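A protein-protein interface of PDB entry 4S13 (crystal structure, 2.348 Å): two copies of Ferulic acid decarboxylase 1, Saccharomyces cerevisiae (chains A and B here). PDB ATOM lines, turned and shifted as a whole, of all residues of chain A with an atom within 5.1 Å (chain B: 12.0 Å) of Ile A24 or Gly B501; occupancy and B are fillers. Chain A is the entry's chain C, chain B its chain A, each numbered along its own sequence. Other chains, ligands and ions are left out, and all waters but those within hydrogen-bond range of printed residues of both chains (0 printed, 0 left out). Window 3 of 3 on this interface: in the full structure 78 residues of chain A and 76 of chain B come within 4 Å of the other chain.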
ATOM      1  N   ASP A  22      18.872  32.769   3.816  1.00  0.00           N
ATOM      2  CA  ASP A  22      17.472  32.829   3.412  1.00  0.00           C
ATOM      3  C   ASP A  22      17.218  31.903   2.233  1.00  0.00           C
ATOM      4  O   ASP A  22      16.335  32.141   1.425  1.00  0.00           O
ATOM      5  CB  ASP A  22      17.061  34.263   3.058  1.00  0.00           C
ATOM      6  CG  ASP A  22      15.540  34.434   2.928  1.00  0.00           C
ATOM      7  OD1 ASP A  22      14.765  33.762   3.650  1.00  0.00           O
ATOM      8  OD2 ASP A  22      15.121  35.245   2.082  1.00  0.00           O
ATOM      9  N   LEU A  23      17.988  30.831   2.143  1.00  0.00           N
ATOM     10  CA  LEU A  23      17.750  29.846   1.111  1.00  0.00           C
ATOM     11  C   LEU A  23      18.172  28.488   1.640  1.00  0.00           C
ATOM     12  O   LEU A  23      19.205  28.379   2.280  1.00  0.00           O
ATOM     13  CB  LEU A  23      18.507  30.220  -0.164  1.00  0.00           C
ATOM     14  CG  LEU A  23      18.220  29.434  -1.443  1.00  0.00           C
ATOM     15  CD1 LEU A  23      17.963  30.373  -2.597  1.00  0.00           C
ATOM     16  CD2 LEU A  23      19.387  28.546  -1.764  1.00  0.00           C
ATOM     17  N   ILE A  24      17.350  27.463   1.425  1.00  0.00           N
ATOM     18  CA  ILE A  24      17.696  26.112   1.875  1.00  0.00           C
ATOM     19  C   ILE A  24      17.827  25.206   0.670  1.00  0.00           C
ATOM     20  O   ILE A  24      16.874  25.019  -0.083  1.00  0.00           O
ATOM     21  CB  ILE A  24      16.650  25.515   2.872  1.00  0.00           C
ATOM     22  CG1 ILE A  24      16.960  25.964   4.290  1.00  0.00           C
ATOM     23  CG2 ILE A  24      16.687  24.002   2.872  1.00  0.00           C
ATOM     24  CD1 ILE A  24      16.122  27.071   4.723  1.00  0.00           C
ATOM     25  N   GLU A  25      19.024  24.664   0.484  1.00  0.00           N
ATOM     26  CA  GLU A  25      19.305  23.799  -0.639  1.00  0.00           C
ATOM     27  C   GLU A  25      18.874  22.395  -0.290  1.00  0.00           C
ATOM     28  O   GLU A  25      19.547  21.698   0.461  1.00  0.00           O
ATOM     29  CB  GLU A  25      20.788  23.841  -0.988  1.00  0.00           C
ATOM     30  CG  GLU A  25      21.306  25.237  -1.299  1.00  0.00           C
ATOM     31  CD  GLU A  25      22.635  25.208  -2.026  1.00  0.00           C
ATOM     32  OE1 GLU A  25      23.660  25.591  -1.424  1.00  0.00           O
ATOM     33  OE2 GLU A  25      22.651  24.803  -3.205  1.00  0.00           O
ATOM     34  N   ILE A  26      17.732  21.987  -0.818  1.00  0.00           N
ATOM     35  CA  ILE A  26      17.186  20.683  -0.492  1.00  0.00           C
ATOM     36  C   ILE A  26      17.728  19.669  -1.483  1.00  0.00           C
ATOM     37  O   ILE A  26      17.309  19.638  -2.640  1.00  0.00           O
ATOM     38  CB  ILE A  26      15.645  20.692  -0.501  1.00  0.00           C
ATOM     39  CG1 ILE A  26      15.115  21.843   0.363  1.00  0.00           C
ATOM     40  CG2 ILE A  26      15.105  19.356  -0.012  1.00  0.00           C
ATOM     41  CD1 ILE A  26      13.585  21.963   0.389  1.00  0.00           C
ATOM     42  N   PRO A  49      12.797  30.670   5.119  1.00  0.00           N
ATOM     43  CA  PRO A  49      13.640  30.765   3.925  1.00  0.00           C
ATOM     44  C   PRO A  49      13.116  29.963   2.726  1.00  0.00           C
ATOM     45  O   PRO A  49      12.390  28.984   2.878  1.00  0.00           O
ATOM     46  CB  PRO A  49      14.972  30.209   4.403  1.00  0.00           C
ATOM     47  CG  PRO A  49      14.980  30.481   5.872  1.00  0.00           C
ATOM     48  CD  PRO A  49      13.579  30.322   6.321  1.00  0.00           C
ATOM     49  N   ALA A  50      13.506  30.399   1.535  1.00  0.00           N
ATOM     50  CA  ALA A  50      13.029  29.811   0.294  1.00  0.00           C
ATOM     51  C   ALA A  50      13.653  28.456   0.018  1.00  0.00           C
ATOM     52  O   ALA A  50      14.851  28.261   0.193  1.00  0.00           O
ATOM     53  CB  ALA A  50      13.298  30.750  -0.865  1.00  0.00           C
ATOM     54  N   PRO A  51      12.825  27.501  -0.409  1.00  0.00           N
ATOM     55  CA  PRO A  51      13.346  26.188  -0.777  1.00  0.00           C
ATOM     56  C   PRO A  51      13.941  26.193  -2.181  1.00  0.00           C
ATOM     57  O   PRO A  51      13.318  26.709  -3.109  1.00  0.00           O
ATOM     58  CB  PRO A  51      12.110  25.295  -0.707  1.00  0.00           C
ATOM     59  CG  PRO A  51      10.981  26.211  -1.001  1.00  0.00           C
ATOM     60  CD  PRO A  51      11.352  27.555  -0.464  1.00  0.00           C
ATOM     61  N   LEU A  52      15.146  25.650  -2.315  1.00  0.00           N
ATOM     62  CA  LEU A  52      15.701  25.328  -3.613  1.00  0.00           C
ATOM     63  C   LEU A  52      15.768  23.817  -3.737  1.00  0.00           C
ATOM     64  O   LEU A  52      16.589  23.173  -3.098  1.00  0.00           O
ATOM     65  CB  LEU A  52      17.090  25.950  -3.795  1.00  0.00           C
ATOM     66  CG  LEU A  52      17.778  25.753  -5.148  1.00  0.00           C
ATOM     67  CD1 LEU A  52      16.915  26.291  -6.274  1.00  0.00           C
ATOM     68  CD2 LEU A  52      19.148  26.422  -5.152  1.00  0.00           C
ATOM     69  N   LYS B 492       4.715  13.992   6.813  1.00  0.00           N
ATOM     70  CA  LYS B 492       6.005  13.687   6.205  1.00  0.00           C
ATOM     71  C   LYS B 492       6.882  14.934   6.122  1.00  0.00           C
ATOM     72  O   LYS B 492       8.065  14.895   6.458  1.00  0.00           O
ATOM     73  CB  LYS B 492       5.820  13.084   4.813  1.00  0.00           C
ATOM     74  CG  LYS B 492       7.113  12.721   4.122  1.00  0.00           C
ATOM     75  CD  LYS B 492       6.863  12.011   2.801  1.00  0.00           C
ATOM     76  CE  LYS B 492       8.176  11.657   2.132  1.00  0.00           C
ATOM     77  NZ  LYS B 492       7.985  10.907   0.861  1.00  0.00           N
ATOM     78  N   VAL B 493       6.295  16.033   5.667  1.00  0.00           N
ATOM     79  CA  VAL B 493       7.002  17.299   5.571  1.00  0.00           C
ATOM     80  C   VAL B 493       7.368  17.808   6.970  1.00  0.00           C
ATOM     81  O   VAL B 493       8.478  18.304   7.194  1.00  0.00           O
ATOM     82  CB  VAL B 493       6.157  18.357   4.816  1.00  0.00           C
ATOM     83  CG1 VAL B 493       6.651  19.764   5.109  1.00  0.00           C
ATOM     84  CG2 VAL B 493       6.152  18.079   3.319  1.00  0.00           C
ATOM     85  N   ASN B 494       6.446  17.675   7.916  1.00  0.00           N
ATOM     86  CA  ASN B 494       6.710  18.114   9.287  1.00  0.00           C
ATOM     87  C   ASN B 494       7.843  17.333   9.948  1.00  0.00           C
ATOM     88  O   ASN B 494       8.650  17.913  10.664  1.00  0.00           O
ATOM     89  CB  ASN B 494       5.445  18.030  10.135  1.00  0.00           C
ATOM     90  CG  ASN B 494       4.648  19.321  10.111  1.00  0.00           C
ATOM     91  OD1 ASN B 494       5.180  20.386   9.789  1.00  0.00           O
ATOM     92  ND2 ASN B 494       3.371  19.236  10.451  1.00  0.00           N
ATOM     93  N   GLU B 495       7.915  16.029   9.694  1.00  0.00           N
ATOM     94  CA  GLU B 495       9.051  15.236  10.154  1.00  0.00           C
ATOM     95  C   GLU B 495      10.330  15.815   9.617  1.00  0.00           C
ATOM     96  O   GLU B 495      11.145  16.379  10.350  1.00  0.00           O
ATOM     97  CB  GLU B 495       8.976  13.791   9.678  1.00  0.00           C
ATOM     98  CG  GLU B 495       7.939  12.908  10.292  1.00  0.00           C
ATOM     99  CD  GLU B 495       7.998  11.521   9.686  1.00  0.00           C
ATOM    100  OE1 GLU B 495       9.073  10.887   9.772  1.00  0.00           O
ATOM    101  OE2 GLU B 495       6.991  11.077   9.097  1.00  0.00           O
ATOM    102  N   ASN B 496      10.470  15.665   8.301  1.00  0.00           N
ATOM    103  CA  ASN B 496      11.715  15.897   7.582  1.00  0.00           C
ATOM    104  C   ASN B 496      12.126  17.358   7.506  1.00  0.00           C
ATOM    105  O   ASN B 496      13.131  17.684   6.887  1.00  0.00           O
ATOM    106  CB  ASN B 496      11.606  15.324   6.164  1.00  0.00           C
ATOM    107  CG  ASN B 496      11.382  13.823   6.159  1.00  0.00           C
ATOM    108  OD1 ASN B 496      11.787  13.128   7.084  1.00  0.00           O
ATOM    109  ND2 ASN B 496      10.739  13.317   5.114  1.00  0.00           N
ATOM    110  N   TRP B 497      11.357  18.230   8.145  1.00  0.00           N
ATOM    111  CA  TRP B 497      11.599  19.661   8.062  1.00  0.00           C
ATOM    112  C   TRP B 497      13.025  20.027   8.483  1.00  0.00           C
ATOM    113  O   TRP B 497      13.686  20.830   7.827  1.00  0.00           O
ATOM    114  CB  TRP B 497      10.583  20.415   8.916  1.00  0.00           C
ATOM    115  CG  TRP B 497      10.470  21.861   8.550  1.00  0.00           C
ATOM    116  CD1 TRP B 497      10.758  22.934   9.339  1.00  0.00           C
ATOM    117  CD2 TRP B 497      10.054  22.391   7.290  1.00  0.00           C
ATOM    118  NE1 TRP B 497      10.537  24.104   8.650  1.00  0.00           N
ATOM    119  CE2 TRP B 497      10.105  23.794   7.388  1.00  0.00           C
ATOM    120  CE3 TRP B 497       9.634  21.814   6.089  1.00  0.00           C
ATOM    121  CZ2 TRP B 497       9.758  24.625   6.334  1.00  0.00           C
ATOM    122  CZ3 TRP B 497       9.289  22.639   5.048  1.00  0.00           C
ATOM    123  CH2 TRP B 497       9.353  24.030   5.173  1.00  0.00           C
ATOM    124  N   LYS B 498      13.504  19.424   9.562  1.00  0.00           N
ATOM    125  CA  LYS B 498      14.847  19.690  10.052  1.00  0.00           C
ATOM    126  C   LYS B 498      15.897  19.110   9.103  1.00  0.00           C
ATOM    127  O   LYS B 498      16.967  19.684   8.913  1.00  0.00           O
ATOM    128  CB  LYS B 498      15.025  19.117  11.461  1.00  0.00           C
ATOM    129  CG  LYS B 498      14.544  20.032  12.592  1.00  0.00           C
ATOM    130  CD  LYS B 498      13.042  20.324  12.506  1.00  0.00           C
ATOM    131  CE  LYS B 498      12.558  21.239  13.635  1.00  0.00           C
ATOM    132  NZ  LYS B 498      11.163  21.731  13.405  1.00  0.00           N
ATOM    133  N   ARG B 499      15.563  17.977   8.495  1.00  0.00           N
ATOM    134  CA  ARG B 499      16.504  17.243   7.671  1.00  0.00           C
ATOM    135  C   ARG B 499      16.686  17.877   6.299  1.00  0.00           C
ATOM    136  O   ARG B 499      17.672  17.609   5.613  1.00  0.00           O
ATOM    137  CB  ARG B 499      16.049  15.794   7.523  1.00  0.00           C
ATOM    138  CG  ARG B 499      17.197  14.829   7.376  1.00  0.00           C
ATOM    139  CD  ARG B 499      16.721  13.396   7.327  1.00  0.00           C
ATOM    140  NE  ARG B 499      15.942  13.123   6.126  1.00  0.00           N
ATOM    141  CZ  ARG B 499      14.820  12.410   6.113  1.00  0.00           C
ATOM    142  NH1 ARG B 499      14.348  11.896   7.244  1.00  0.00           N
ATOM    143  NH2 ARG B 499      14.170  12.212   4.971  1.00  0.00           N
ATOM    144  N   TYR B 500      15.735  18.709   5.893  1.00  0.00           N
ATOM    145  CA  TYR B 500      15.856  19.439   4.638  1.00  0.00           C
ATOM    146  C   TYR B 500      16.888  20.544   4.781  1.00  0.00           C
ATOM    147  O   TYR B 500      17.604  20.862   3.836  1.00  0.00           O
ATOM    148  CB  TYR B 500      14.520  20.057   4.221  1.00  0.00           C
ATOM    149  CG  TYR B 500      13.438  19.081   3.854  1.00  0.00           C
ATOM    150  CD1 TYR B 500      13.742  17.828   3.355  1.00  0.00           C
ATOM    151  CD2 TYR B 500      12.106  19.419   4.003  1.00  0.00           C
ATOM    152  CE1 TYR B 500      12.745  16.939   3.020  1.00  0.00           C
ATOM    153  CE2 TYR B 500      11.109  18.541   3.668  1.00  0.00           C
ATOM    154  CZ  TYR B 500      11.434  17.303   3.176  1.00  0.00           C
ATOM    155  OH  TYR B 500      10.436  16.420   2.842  1.00  0.00           O
ATOM    156  N   GLY B 501      16.937  21.140   5.970  1.00  0.00           N
ATOM    157  CA  GLY B 501      17.836  22.245   6.248  1.00  0.00           C
ATOM    158  C   GLY B 501      17.205  23.346   7.082  1.00  0.00           C
ATOM    159  O   GLY B 501      17.914  24.190   7.623  1.00  0.00           O
ATOM    160  N   TYR B 502      15.878  23.346   7.179  1.00  0.00           N
ATOM    161  CA  TYR B 502      15.161  24.318   8.012  1.00  0.00           C
ATOM    162  C   TYR B 502      15.435  24.148   9.508  1.00  0.00           C
ATOM    163  O   TYR B 502      15.912  23.105   9.955  1.00  0.00           O
ATOM    164  CB  TYR B 502      13.650  24.235   7.766  1.00  0.00           C
ATOM    165  CG  TYR B 502      13.232  24.820   6.446  1.00  0.00           C
ATOM    166  CD1 TYR B 502      12.991  26.177   6.315  1.00  0.00           C
ATOM    167  CD2 TYR B 502      13.111  24.020   5.323  1.00  0.00           C
ATOM    168  CE1 TYR B 502      12.627  26.722   5.105  1.00  0.00           C
ATOM    169  CE2 TYR B 502      12.747  24.554   4.105  1.00  0.00           C
ATOM    170  CZ  TYR B 502      12.507  25.903   4.003  1.00  0.00           C
ATOM    171  OH  TYR B 502      12.144  26.433   2.793  1.00  0.00           O
ATOM    172  N   LYS B 503      15.114  25.186  10.273  1.00  0.00           N
ATOM    173  CA  LYS B 503      15.435  25.229  11.693  1.00  0.00           C
ATOM    174  C   LYS B 503      14.214  24.926  12.553  1.00  0.00           C
ATOM    175  O   LYS B 503      14.347  24.670  13.752  1.00  0.00           O
ATOM    176  CB  LYS B 503      16.016  26.597  12.064  1.00  0.00           C
ATOM    177  CG  LYS B 503      17.529  26.613  12.242  1.00  0.00           C
ATOM    178  CD  LYS B 503      18.259  26.048  11.026  1.00  0.00           C
ATOM    179  CE  LYS B 503      19.735  25.799  11.333  1.00  0.00           C
ATOM    180  NZ  LYS B 503      20.435  25.066  10.230  1.00  0.00           N
ATOM    181  OXT LYS B 503      13.074  24.930  12.075  1.00  0.00           O
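Of the 9 printed residues of chain A, 6 touch a printed residue of chain B.
Hydrophobic or aromatic side chains of chain B within 4 Å of the printed part of chain A: Tyr B500 and Tyr B502.
Among the printed residues, 8 pairs touch across the chains.
Among the printed residues, no Asp or Glu carboxylate lies within 4 Å of a Lys or Arg side-chain nitrogen of the other chain.
The backbone carbonyl oxygen (O) of Pro A49 sits at hydrogen-bond distance from the side-chain hydroxyl (OH) of Tyr B502 (2.6 Å).
OH of Tyr B502 lies close to N of Pro A51, at 3.4 Å.
No position is printed for both chains.
Of the 8 pairs that touch across the chains among the printed residues, none has its exchanged pair printed and touching as well.
Ile A24 touches Tyr B500 (CG2 to O, 3.4 Å).
Gly B501 touches Ile A24.
Ile A24 touches Tyr B502.
Glu A25 touches Tyr B500 (O to O, 3.98 Å).
Tyr B500 touches Ile A26.
Ala A50 touches Tyr B502 (C to OH, 3.8 Å).
Of chain B, only Tyr B500, Gly B501 and Tyr B502 come within 4 Å of Ile A24.
Gly B501 touches just one residue of chain A: Ile A24 (3.8 Å).
No residue of chain B comes within 4 Å of Leu A23.
Of chain B, only Tyr B500 (3.9 Å) comes within 4 Å of Ile A26.
Pro A49 touches just one residue of chain B: Tyr B502 (2.6 Å).
Ala A50 touches one residue of chain B.
Of the printed residues of chain B, Glu A25 touches Tyr B500 (3.98 Å).
Printed residues of chain A within 4 Å of Tyr B502: Ile A24, Pro A49, Ala A50 and Pro A51.
Printed residues of chain A within 4 Å of Tyr B500: Ile A24, Glu A25 and Ile A26.
The nearest residue of chain B that does not touch Ile A24 is Lys B503 (5.9 Å).
The nearest printed residue of chain A that does not touch Gly B501 is Ile A26 (5.9 Å).
The nearest printed residue of chain A that does not touch Tyr B500 is Leu A52 (7.4 Å).
The backbone NH (N) of Tyr B502 sits at hydrogen-bond distance from the backbone carbonyl oxygen (O) of Trp B497 (3.4 Å).
N of Ala A50 sits at hydrogen-bond distance from O of Asp A22 (3.3 Å).
O of Leu A52 lies within hydrogen-bond range of N of Ile A26, 2.8 Å away.
N of Leu A52 sits at hydrogen-bond distance from O of Ile A24, at 2.9 Å.
The backbone NH of Ile A24 sits at hydrogen-bond distance from the backbone carbonyl oxygen of Ala A50, 2.9 Å away.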
